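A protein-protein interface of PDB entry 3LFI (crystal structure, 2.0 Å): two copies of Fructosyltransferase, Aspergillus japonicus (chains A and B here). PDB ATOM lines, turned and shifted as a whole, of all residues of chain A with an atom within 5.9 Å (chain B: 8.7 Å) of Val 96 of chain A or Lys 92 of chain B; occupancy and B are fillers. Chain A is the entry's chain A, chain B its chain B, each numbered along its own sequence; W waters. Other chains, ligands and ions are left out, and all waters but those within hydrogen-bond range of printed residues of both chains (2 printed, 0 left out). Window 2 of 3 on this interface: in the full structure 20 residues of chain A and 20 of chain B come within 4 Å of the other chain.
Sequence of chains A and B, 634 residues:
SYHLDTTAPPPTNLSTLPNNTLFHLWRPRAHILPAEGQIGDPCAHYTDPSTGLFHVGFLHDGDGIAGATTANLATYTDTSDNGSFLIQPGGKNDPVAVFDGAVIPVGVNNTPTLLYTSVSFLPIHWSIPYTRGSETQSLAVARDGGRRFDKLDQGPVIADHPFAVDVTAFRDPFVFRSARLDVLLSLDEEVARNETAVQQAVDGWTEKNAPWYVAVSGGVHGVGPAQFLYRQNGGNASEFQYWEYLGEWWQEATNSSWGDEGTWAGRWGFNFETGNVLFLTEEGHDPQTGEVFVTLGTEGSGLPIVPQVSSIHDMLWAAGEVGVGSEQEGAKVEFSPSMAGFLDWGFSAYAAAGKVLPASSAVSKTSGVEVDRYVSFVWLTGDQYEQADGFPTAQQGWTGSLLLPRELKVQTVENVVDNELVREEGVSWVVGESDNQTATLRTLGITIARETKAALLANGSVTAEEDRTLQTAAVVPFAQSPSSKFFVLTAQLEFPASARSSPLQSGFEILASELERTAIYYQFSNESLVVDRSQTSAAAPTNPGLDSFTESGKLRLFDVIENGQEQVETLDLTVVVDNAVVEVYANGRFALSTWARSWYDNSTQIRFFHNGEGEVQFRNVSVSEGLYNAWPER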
ATOM      1  N   PRO A  89     -13.440  17.815 -31.100  1.00  0.00           N
ATOM      2  CA  PRO A  89     -12.984  17.475 -29.751  1.00  0.00           C
ATOM      3  C   PRO A  89     -11.669  18.120 -29.328  1.00  0.00           C
ATOM      4  O   PRO A  89     -10.990  18.777 -30.125  1.00  0.00           O
ATOM      5  CB  PRO A  89     -12.909  15.953 -29.793  1.00  0.00           C
ATOM      6  CG  PRO A  89     -12.541  15.683 -31.220  1.00  0.00           C
ATOM      7  CD  PRO A  89     -13.442  16.624 -31.967  1.00  0.00           C
ATOM      8  N   GLY A  90     -11.314  17.924 -28.065  1.00  0.00           N
ATOM      9  CA  GLY A  90     -10.087  18.496 -27.542  1.00  0.00           C
ATOM     10  C   GLY A  90     -10.361  19.502 -26.437  1.00  0.00           C
ATOM     11  O   GLY A  90      -9.437  20.080 -25.865  1.00  0.00           O
ATOM     12  N   GLY A  91     -11.634  19.725 -26.146  1.00  0.00           N
ATOM     13  CA  GLY A  91     -11.996  20.644 -25.081  1.00  0.00           C
ATOM     14  C   GLY A  91     -11.846  19.898 -23.768  1.00  0.00           C
ATOM     15  O   GLY A  91     -11.483  18.717 -23.766  1.00  0.00           O
ATOM     16  N   LYS A  92     -12.116  20.557 -22.645  1.00  0.00           N
ATOM     17  CA  LYS A  92     -11.977  19.871 -21.369  1.00  0.00           C
ATOM     18  C   LYS A  92     -13.116  18.874 -21.146  1.00  0.00           C
ATOM     19  O   LYS A  92     -12.906  17.838 -20.527  1.00  0.00           O
ATOM     20  CB  LYS A  92     -11.877  20.882 -20.210  1.00  0.00           C
ATOM     21  CG  LYS A  92     -12.555  22.213 -20.464  1.00  0.00           C
ATOM     22  CD  LYS A  92     -11.593  23.404 -20.269  1.00  0.00           C
ATOM     23  CE  LYS A  92     -10.925  23.403 -18.900  1.00  0.00           C
ATOM     24  NZ  LYS A  92     -10.253  24.705 -18.570  1.00  0.00           N
ATOM     25  N   ASP A  94     -14.877  17.395 -23.741  1.00  0.00           N
ATOM     26  CA  ASP A  94     -14.811  16.413 -24.827  1.00  0.00           C
ATOM     27  C   ASP A  94     -13.374  16.164 -25.278  1.00  0.00           C
ATOM     28  O   ASP A  94     -13.046  16.328 -26.452  1.00  0.00           O
ATOM     29  CB  ASP A  94     -15.648  16.878 -26.033  1.00  0.00           C
ATOM     30  CG  ASP A  94     -15.376  18.331 -26.439  1.00  0.00           C
ATOM     31  OD1 ASP A  94     -14.385  18.936 -25.967  1.00  0.00           O
ATOM     32  OD2 ASP A  94     -16.169  18.869 -27.248  1.00  0.00           O
ATOM     33  N   PRO A  95     -12.501  15.729 -24.353  1.00  0.00           N
ATOM     34  CA  PRO A  95     -11.111  15.487 -24.734  1.00  0.00           C
ATOM     35  C   PRO A  95     -10.922  14.389 -25.770  1.00  0.00           C
ATOM     36  O   PRO A  95      -9.966  14.433 -26.539  1.00  0.00           O
ATOM     37  CB  PRO A  95     -10.442  15.147 -23.410  1.00  0.00           C
ATOM     38  CG  PRO A  95     -11.549  14.442 -22.657  1.00  0.00           C
ATOM     39  CD  PRO A  95     -12.769  15.270 -22.980  1.00  0.00           C
ATOM     40  N   VAL A  96     -11.836  13.423 -25.803  1.00  0.00           N
ATOM     41  CA  VAL A  96     -11.717  12.307 -26.734  1.00  0.00           C
ATOM     42  C   VAL A  96     -12.530  12.443 -28.021  1.00  0.00           C
ATOM     43  O   VAL A  96     -12.003  12.194 -29.105  1.00  0.00           O
ATOM     44  CB  VAL A  96     -12.068  10.975 -26.025  1.00  0.00           C
ATOM     45  CG1 VAL A  96     -12.050   9.810 -27.028  1.00  0.00           C
ATOM     46  CG2 VAL A  96     -11.047  10.702 -24.930  1.00  0.00           C
ATOM     47  N   ALA A  97     -13.796  12.842 -27.924  1.00  0.00           N
ATOM     48  CA  ALA A  97     -14.603  12.996 -29.133  1.00  0.00           C
ATOM     49  C   ALA A  97     -15.861  13.834 -28.955  1.00  0.00           C
ATOM     50  O   ALA A  97     -16.256  14.177 -27.838  1.00  0.00           O
ATOM     51  CB  ALA A  97     -14.983  11.629 -29.676  1.00  0.00           C
ATOM     52  N   VAL A  98     -16.470  14.170 -30.083  1.00  0.00           N
ATOM     53  CA  VAL A  98     -17.710  14.925 -30.107  1.00  0.00           C
ATOM     54  C   VAL A  98     -18.781  14.065 -30.795  1.00  0.00           C
ATOM     55  O   VAL A  98     -18.677  13.783 -31.982  1.00  0.00           O
ATOM     56  CB  VAL A  98     -17.532  16.247 -30.883  1.00  0.00           C
ATOM     57  CG1 VAL A  98     -18.882  16.889 -31.133  1.00  0.00           C
ATOM     58  CG2 VAL A  98     -16.632  17.201 -30.089  1.00  0.00           C
ATOM     59  N   VAL A 119     -17.467  13.521 -25.293  1.00  0.00           N
ATOM     60  CA  VAL A 119     -16.868  12.244 -24.911  1.00  0.00           C
ATOM     61  C   VAL A 119     -15.479  12.324 -24.298  1.00  0.00           C
ATOM     62  O   VAL A 119     -14.565  12.947 -24.863  1.00  0.00           O
ATOM     63  CB  VAL A 119     -16.810  11.306 -26.124  1.00  0.00           C
ATOM     64  CG1 VAL A 119     -16.248   9.951 -25.722  1.00  0.00           C
ATOM     65  CG2 VAL A 119     -18.204  11.156 -26.708  1.00  0.00           C
ATOM     66  N   SER A 120     -15.321  11.656 -23.157  1.00  0.00           N
ATOM     67  CA  SER A 120     -14.052  11.654 -22.442  1.00  0.00           C
ATOM     68  C   SER A 120     -13.354  10.302 -22.354  1.00  0.00           C
ATOM     69  O   SER A 120     -12.191  10.233 -21.956  1.00  0.00           O
ATOM     70  CB  SER A 120     -14.257  12.204 -21.029  1.00  0.00           C
ATOM     71  OG  SER A 120     -14.722  13.541 -21.085  1.00  0.00           O
ATOM     72  N   PHE A 121     -14.052   9.231 -22.714  1.00  0.00           N
ATOM     73  CA  PHE A 121     -13.459   7.890 -22.657  1.00  0.00           C
ATOM     74  C   PHE A 121     -14.024   6.975 -23.738  1.00  0.00           C
ATOM     75  O   PHE A 121     -15.192   7.096 -24.123  1.00  0.00           O
ATOM     76  CB  PHE A 121     -13.728   7.254 -21.291  1.00  0.00           C
ATOM     77  CG  PHE A 121     -13.161   8.032 -20.135  1.00  0.00           C
ATOM     78  CD1 PHE A 121     -11.852   7.818 -19.708  1.00  0.00           C
ATOM     79  CD2 PHE A 121     -13.931   8.994 -19.489  1.00  0.00           C
ATOM     80  CE1 PHE A 121     -11.318   8.557 -18.647  1.00  0.00           C
ATOM     81  CE2 PHE A 121     -13.408   9.739 -18.431  1.00  0.00           C
ATOM     82  CZ  PHE A 121     -12.094   9.517 -18.010  1.00  0.00           C
ATOM     83  N   LEU A 122     -13.179   6.068 -24.223  1.00  0.00           N
ATOM     84  CA  LEU A 122     -13.555   5.077 -25.233  1.00  0.00           C
ATOM     85  C   LEU A 122     -12.814   3.804 -24.852  1.00  0.00           C
ATOM     86  O   LEU A 122     -11.764   3.865 -24.204  1.00  0.00           O
ATOM     87  CB  LEU A 122     -13.113   5.508 -26.633  1.00  0.00           C
ATOM     88  CG  LEU A 122     -13.835   6.640 -27.360  1.00  0.00           C
ATOM     89  CD1 LEU A 122     -13.025   6.994 -28.612  1.00  0.00           C
ATOM     90  CD2 LEU A 122     -15.259   6.218 -27.742  1.00  0.00           C
ATOM     91  N   GLN B  88      -0.545  14.816  -9.585  1.00  0.00           N
ATOM     92  CA  GLN B  88      -0.543  16.170 -10.126  1.00  0.00           C
ATOM     93  C   GLN B  88      -1.644  16.352 -11.183  1.00  0.00           C
ATOM     94  O   GLN B  88      -2.188  15.373 -11.687  1.00  0.00           O
ATOM     95  CB  GLN B  88       0.842  16.463 -10.719  1.00  0.00           C
ATOM     96  CG  GLN B  88       1.980  16.323  -9.699  1.00  0.00           C
ATOM     97  CD  GLN B  88       3.347  16.681 -10.268  1.00  0.00           C
ATOM     98  OE1 GLN B  88       3.961  15.888 -10.976  1.00  0.00           O
ATOM     99  NE2 GLN B  88       3.824  17.886  -9.963  1.00  0.00           N
ATOM    100  N   PRO B  89      -1.993  17.612 -11.513  1.00  0.00           N
ATOM    101  CA  PRO B  89      -3.030  17.886 -12.509  1.00  0.00           C
ATOM    102  C   PRO B  89      -2.623  17.588 -13.951  1.00  0.00           C
ATOM    103  O   PRO B  89      -1.457  17.298 -14.236  1.00  0.00           O
ATOM    104  CB  PRO B  89      -3.340  19.361 -12.286  1.00  0.00           C
ATOM    105  CG  PRO B  89      -2.030  19.907 -11.816  1.00  0.00           C
ATOM    106  CD  PRO B  89      -1.586  18.858 -10.839  1.00  0.00           C
ATOM    107  N   GLY B  90      -3.598  17.670 -14.850  1.00  0.00           N
ATOM    108  CA  GLY B  90      -3.346  17.393 -16.253  1.00  0.00           C
ATOM    109  C   GLY B  90      -4.072  16.144 -16.723  1.00  0.00           C
ATOM    110  O   GLY B  90      -3.904  15.702 -17.862  1.00  0.00           O
ATOM    111  N   GLY B  91      -4.871  15.554 -15.839  1.00  0.00           N
ATOM    112  CA  GLY B  91      -5.625  14.371 -16.212  1.00  0.00           C
ATOM    113  C   GLY B  91      -6.895  14.845 -16.884  1.00  0.00           C
ATOM    114  O   GLY B  91      -7.080  16.048 -17.052  1.00  0.00           O
ATOM    115  N   LYS B  92      -7.770  13.923 -17.276  1.00  0.00           N
ATOM    116  CA  LYS B  92      -9.020  14.309 -17.921  1.00  0.00           C
ATOM    117  C   LYS B  92      -9.982  14.967 -16.938  1.00  0.00           C
ATOM    118  O   LYS B  92     -10.713  15.879 -17.303  1.00  0.00           O
ATOM    119  CB  LYS B  92      -9.704  13.090 -18.557  1.00  0.00           C
ATOM    120  CG  LYS B  92      -9.048  12.590 -19.840  1.00  0.00           C
ATOM    121  CD  LYS B  92      -9.659  11.262 -20.276  1.00  0.00           C
ATOM    122  CE  LYS B  92      -8.941  10.673 -21.467  1.00  0.00           C
ATOM    123  NZ  LYS B  92      -9.513   9.340 -21.780  1.00  0.00           N
ATOM    124  N   ASN B  93      -9.973  14.508 -15.690  1.00  0.00           N
ATOM    125  CA  ASN B  93     -10.871  15.047 -14.672  1.00  0.00           C
ATOM    126  C   ASN B  93     -10.341  16.309 -13.998  1.00  0.00           C
ATOM    127  O   ASN B  93     -11.128  17.133 -13.527  1.00  0.00           O
ATOM    128  CB  ASN B  93     -11.135  14.001 -13.580  1.00  0.00           C
ATOM    129  CG  ASN B  93     -11.588  12.673 -14.142  1.00  0.00           C
ATOM    130  OD1 ASN B  93     -12.125  12.613 -15.242  1.00  0.00           O
ATOM    131  ND2 ASN B  93     -11.379  11.600 -13.382  1.00  0.00           N
ATOM    132  N   ASP B  94      -9.014  16.428 -13.941  1.00  0.00           N
ATOM    133  CA  ASP B  94      -8.340  17.557 -13.306  1.00  0.00           C
ATOM    134  C   ASP B  94      -7.378  18.245 -14.268  1.00  0.00           C
ATOM    135  O   ASP B  94      -6.189  18.355 -13.988  1.00  0.00           O
ATOM    136  CB  ASP B  94      -7.561  17.076 -12.067  1.00  0.00           C
ATOM    137  CG  ASP B  94      -6.696  15.836 -12.345  1.00  0.00           C
ATOM    138  OD1 ASP B  94      -6.415  15.523 -13.525  1.00  0.00           O
ATOM    139  OD2 ASP B  94      -6.283  15.175 -11.371  1.00  0.00           O
ATOM    140  N   PRO B  95      -7.886  18.736 -15.412  1.00  0.00           N
ATOM    141  CA  PRO B  95      -6.969  19.389 -16.343  1.00  0.00           C
ATOM    142  C   PRO B  95      -6.294  20.629 -15.778  1.00  0.00           C
ATOM    143  O   PRO B  95      -5.158  20.924 -16.135  1.00  0.00           O
ATOM    144  CB  PRO B  95      -7.858  19.705 -17.549  1.00  0.00           C
ATOM    145  CG  PRO B  95      -9.211  19.885 -16.949  1.00  0.00           C
ATOM    146  CD  PRO B  95      -9.275  18.791 -15.898  1.00  0.00           C
ATOM    147  N   VAL B  96      -6.980  21.333 -14.881  1.00  0.00           N
ATOM    148  CA  VAL B  96      -6.444  22.565 -14.308  1.00  0.00           C
ATOM    149  C   VAL B  96      -5.694  22.416 -12.983  1.00  0.00           C
ATOM    150  O   VAL B  96      -4.613  22.974 -12.823  1.00  0.00           O
ATOM    151  CB  VAL B  96      -7.572  23.614 -14.154  1.00  0.00           C
ATOM    152  CG1 VAL B  96      -7.034  24.896 -13.500  1.00  0.00           C
ATOM    153  CG2 VAL B  96      -8.139  23.947 -15.532  1.00  0.00           C
ATOM    154  N   TYR B 116     -10.376  12.800  -4.199  1.00  0.00           N
ATOM    155  CA  TYR B 116      -9.911  14.183  -4.182  1.00  0.00           C
ATOM    156  C   TYR B 116     -10.671  15.105  -5.116  1.00  0.00           C
ATOM    157  O   TYR B 116     -11.364  14.660  -6.037  1.00  0.00           O
ATOM    158  CB  TYR B 116      -8.419  14.229  -4.545  1.00  0.00           C
ATOM    159  CG  TYR B 116      -8.138  13.949  -6.012  1.00  0.00           C
ATOM    160  CD1 TYR B 116      -7.896  14.994  -6.907  1.00  0.00           C
ATOM    161  CD2 TYR B 116      -8.127  12.644  -6.505  1.00  0.00           C
ATOM    162  CE1 TYR B 116      -7.645  14.744  -8.265  1.00  0.00           C
ATOM    163  CE2 TYR B 116      -7.878  12.380  -7.857  1.00  0.00           C
ATOM    164  CZ  TYR B 116      -7.636  13.434  -8.726  1.00  0.00           C
ATOM    165  OH  TYR B 116      -7.368  13.186 -10.045  1.00  0.00           O
ATOM    166  N   SER B 118     -10.875  17.186  -8.123  1.00  0.00           N
ATOM    167  CA  SER B 118     -10.228  17.392  -9.407  1.00  0.00           C
ATOM    168  C   SER B 118     -10.823  18.680  -9.965  1.00  0.00           C
ATOM    169  O   SER B 118     -12.044  18.831 -10.038  1.00  0.00           O
ATOM    170  CB  SER B 118     -10.514  16.204 -10.323  1.00  0.00           C
ATOM    171  OG  SER B 118     -11.813  15.700 -10.085  1.00  0.00           O
ATOM    172  N   VAL B 119      -9.943  19.606 -10.334  1.00  0.00           N
ATOM    173  CA  VAL B 119     -10.344  20.912 -10.833  1.00  0.00           C
ATOM    174  C   VAL B 119     -10.170  21.112 -12.335  1.00  0.00           C
ATOM    175  O   VAL B 119      -9.097  20.848 -12.900  1.00  0.00           O
ATOM    176  CB  VAL B 119      -9.570  22.003 -10.089  1.00  0.00           C
ATOM    177  CG1 VAL B 119      -9.991  23.382 -10.575  1.00  0.00           C
ATOM    178  CG2 VAL B 119      -9.815  21.859  -8.603  1.00  0.00           C
ATOM    179  N   SER B 120     -11.233  21.617 -12.960  1.00  0.00           N
ATOM    180  CA  SER B 120     -11.255  21.854 -14.394  1.00  0.00           C
ATOM    181  C   SER B 120     -11.396  23.317 -14.824  1.00  0.00           C
ATOM    182  O   SER B 120     -11.244  23.630 -16.009  1.00  0.00           O
ATOM    183  CB  SER B 120     -12.384  21.033 -15.015  1.00  0.00           C
ATOM    184  OG  SER B 120     -12.202  19.658 -14.724  1.00  0.00           O
ATOM    185  N   PHE B 121     -11.690  24.207 -13.879  1.00  0.00           N
ATOM    186  CA  PHE B 121     -11.841  25.637 -14.188  1.00  0.00           C
ATOM    187  C   PHE B 121     -11.461  26.529 -13.007  1.00  0.00           C
ATOM    188  O   PHE B 121     -11.691  26.175 -11.847  1.00  0.00           O
ATOM    189  CB  PHE B 121     -13.290  25.951 -14.566  1.00  0.00           C
ATOM    190  CG  PHE B 121     -13.807  25.148 -15.724  1.00  0.00           C
ATOM    191  CD1 PHE B 121     -13.663  25.610 -17.028  1.00  0.00           C
ATOM    192  CD2 PHE B 121     -14.399  23.905 -15.508  1.00  0.00           C
ATOM    193  CE1 PHE B 121     -14.096  24.844 -18.104  1.00  0.00           C
ATOM    194  CE2 PHE B 121     -14.832  23.133 -16.573  1.00  0.00           C
ATOM    195  CZ  PHE B 121     -14.681  23.601 -17.874  1.00  0.00           C
ATOM    196  N   GLY B 133     -18.996  22.678 -13.050  1.00  0.00           N
ATOM    197  CA  GLY B 133     -17.961  21.708 -13.349  1.00  0.00           C
ATOM    198  C   GLY B 133     -16.583  22.090 -12.850  1.00  0.00           C
ATOM    199  O   GLY B 133     -15.610  21.396 -13.133  1.00  0.00           O
ATOM    200  N   THR B 136     -14.878  18.649  -9.019  1.00  0.00           N
ATOM    201  CA  THR B 136     -15.525  17.342  -8.984  1.00  0.00           C
ATOM    202  C   THR B 136     -14.679  16.464  -8.076  1.00  0.00           C
ATOM    203  O   THR B 136     -13.531  16.801  -7.778  1.00  0.00           O
ATOM    204  CB  THR B 136     -15.619  16.687 -10.388  1.00  0.00           C
ATOM    205  OG1 THR B 136     -14.302  16.462 -10.922  1.00  0.00           O
ATOM    206  CG2 THR B 136     -16.419  17.592 -11.339  1.00  0.00           C
ATOM    207  N   SER B 138     -12.817  12.924  -7.643  1.00  0.00           N
ATOM    208  CA  SER B 138     -12.337  11.756  -8.378  1.00  0.00           C
ATOM    209  C   SER B 138     -11.541  10.797  -7.506  1.00  0.00           C
ATOM    210  O   SER B 138     -11.148  11.140  -6.392  1.00  0.00           O
ATOM    211  CB  SER B 138     -11.480  12.208  -9.569  1.00  0.00           C
ATOM    212  OG  SER B 138     -12.236  13.023 -10.452  1.00  0.00           O
ATOM    213  N   LYS B 151      -4.484   7.878 -10.974  1.00  0.00           N
ATOM    214  CA  LYS B 151      -5.884   8.238 -11.143  1.00  0.00           C
ATOM    215  C   LYS B 151      -6.627   7.073 -11.791  1.00  0.00           C
ATOM    216  O   LYS B 151      -6.109   6.454 -12.707  1.00  0.00           O
ATOM    217  CB  LYS B 151      -5.988   9.469 -12.043  1.00  0.00           C
ATOM    218  CG  LYS B 151      -5.184  10.661 -11.544  1.00  0.00           C
ATOM    219  CD  LYS B 151      -5.112  11.761 -12.584  1.00  0.00           C
ATOM    220  CE  LYS B 151      -4.202  12.890 -12.088  1.00  0.00           C
ATOM    221  NZ  LYS B 151      -4.115  14.008 -13.054  1.00  0.00           N
ATOM    222  N   LEU B 152      -7.825   6.755 -11.312  1.00  0.00           N
ATOM    223  CA  LEU B 152      -8.558   5.671 -11.949  1.00  0.00           C
ATOM    224  C   LEU B 152      -8.937   6.177 -13.333  1.00  0.00           C
ATOM    225  O   LEU B 152      -9.223   7.371 -13.519  1.00  0.00           O
ATOM    226  CB  LEU B 152      -9.813   5.284 -11.153  1.00  0.00           C
ATOM    227  CG  LEU B 152      -9.549   4.555  -9.835  1.00  0.00           C
ATOM    228  CD1 LEU B 152     -10.875   4.118  -9.208  1.00  0.00           C
ATOM    229  CD2 LEU B 152      -8.664   3.346 -10.082  1.00  0.00           C
ATOM    230  N   ASP B 153      -8.911   5.275 -14.306  1.00  0.00           N
ATOM    231  CA  ASP B 153      -9.230   5.630 -15.683  1.00  0.00           C
ATOM    232  C   ASP B 153     -10.726   5.784 -15.995  1.00  0.00           C
ATOM    233  O   ASP B 153     -11.319   4.986 -16.725  1.00  0.00           O
ATOM    234  CB  ASP B 153      -8.594   4.608 -16.632  1.00  0.00           C
ATOM    235  CG  ASP B 153      -8.625   5.055 -18.076  1.00  0.00           C
ATOM    236  OD1 ASP B 153      -8.442   6.267 -18.343  1.00  0.00           O
ATOM    237  OD2 ASP B 153      -8.813   4.184 -18.953  1.00  0.00           O
ATOM    238  N   GLN B 154     -11.326   6.814 -15.418  1.00  0.00           N
ATOM    239  CA  GLN B 154     -12.724   7.148 -15.655  1.00  0.00           C
ATOM    240  C   GLN B 154     -13.035   8.525 -15.084  1.00  0.00           C
ATOM    241  O   GLN B 154     -12.167   9.163 -14.487  1.00  0.00           O
ATOM    242  CB  GLN B 154     -13.676   6.077 -15.090  1.00  0.00           C
ATOM    243  CG  GLN B 154     -13.462   5.629 -13.665  1.00  0.00           C
ATOM    244  CD  GLN B 154     -13.917   6.646 -12.664  1.00  0.00           C
ATOM    245  OE1 GLN B 154     -13.214   7.622 -12.410  1.00  0.00           O
ATOM    246  NE2 GLN B 154     -15.108   6.439 -12.088  1.00  0.00           N
ATOM    247  N   GLY B 155     -14.260   8.992 -15.293  1.00  0.00           N
ATOM    248  CA  GLY B 155     -14.651  10.307 -14.805  1.00  0.00           C
ATOM    249  C   GLY B 155     -14.781  10.370 -13.299  1.00  0.00           C
ATOM    250  O   GLY B 155     -14.609   9.354 -12.623  1.00  0.00           O
ATOM    251  N   PRO B 156     -15.079  11.552 -12.736  1.00  0.00           N
ATOM    252  CA  PRO B 156     -15.230  11.709 -11.282  1.00  0.00           C
ATOM    253  C   PRO B 156     -16.364  10.839 -10.735  1.00  0.00           C
ATOM    254  O   PRO B 156     -17.324  10.583 -11.451  1.00  0.00           O
ATOM    255  CB  PRO B 156     -15.515  13.207 -11.118  1.00  0.00           C
ATOM    256  CG  PRO B 156     -16.146  13.602 -12.445  1.00  0.00           C
ATOM    257  CD  PRO B 156     -15.310  12.827 -13.443  1.00  0.00           C
HETATM  258  O   HOH W   1     -10.432  17.110 -19.724  1.00  0.00           O
HETATM  259  O   HOH W   2     -10.396   6.864 -23.131  1.00  0.00           O
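The side-chain amino group (NZ) of Lys 92 of chain B lies within hydrogen-bond range of the backbone carbonyl oxygen (O) of Ser 120 of chain A (2.8 Å). The side-chain amino group (NZ) of Lys 92 of chain A sits close to the backbone carbonyl oxygen (O) of Ser 120 of chain B, at 2.9 Å.
O of Val 119 of chain B is in hydrogen-bond range of N of Val 96 of chain B, at 2.9 Å. N of Val 96 of chain A lies within hydrogen-bond range of O of Val 119 of chain A, at 2.9 Å. ND2 of Asn 93 of chain B is in hydrogen-bond range of O of Gln 154 of chain B (2.8 Å). OG of Ser 120 of chain B lies within hydrogen-bond range of O of Asn 93 of chain B (3.0 Å).
Lys 92 of chain A touches Val 96 of chain B. Phe 121 of chain B touches Lys 92 of chain A (CE1 to CE, 3.6 Å). Val 96 of chain A touches Lys 92 of chain B. CD1 of Phe 121 of chain A touches NZ of Lys 92 of chain B, 3.5 Å away. Phe 121 of chain A touches Asp 153 of chain B (CE1 to OD1, 3.7 Å). Phe 121 of chain A touches Gln 154 of chain B (CZ to C, 3.2 Å). Phe 121 of chain A touches Gly 155 of chain B.
Pro 95 of chain A touches none of the printed residues of chain B. Of chain B, only Lys 92 (3.8 Å) comes within 4 Å of Val 96 of chain A. Of chain A, only Val 96 (3.8 Å), Ser 120 (2.8 Å) and Phe 121 (3.5 Å) come within 4 Å of Lys 92 of chain B. Of the printed residues of chain A, Val 96 of chain B touches Lys 92. Of the printed residues of chain A, Ser 120 of chain B touches Lys 92 (2.9 Å). Lys 151 of chain B touches none of the printed residues of chain A. The nearest residue of chain B that does not touch Val 96 of chain A is Asp 153 of chain B (8.4 Å).
Hydrophobic or aromatic side chains of chain B that line the printed part of chain A: Val 96 and Phe 121. Along chain A the printed residues that touch a printed residue of chain B span positions 92 to 121. Among the printed residues, 9 pairs touch across the chains. Among the printed residues, no Asp or Glu carboxylate lies within 4 Å of a Lys or Arg side-chain nitrogen of the other chain.
Lys 92 of chain A touches Val 96 of chain B, and with the chains exchanged Val 96 of chain A touches Lys 92 of chain B. Lys 92 of chain A touches Ser 120 of chain B, and with the chains exchanged Ser 120 of chain A touches Lys 92 of chain B. Lys 92 of chain A touches Phe 121 of chain B, and with the chains exchanged Phe 121 of chain A touches Lys 92 of chain B.
Water W1 lies within hydrogen-bond range of the backbone carbonyl oxygen of Lys 92 of chain A and the backbone carbonyl oxygen of Lys 92 of chain B. Water W2 lies within hydrogen-bond range of NZ of Lys 92 of chain B (3.0 Å) and N of Leu 122 of chain A (3.1 Å).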
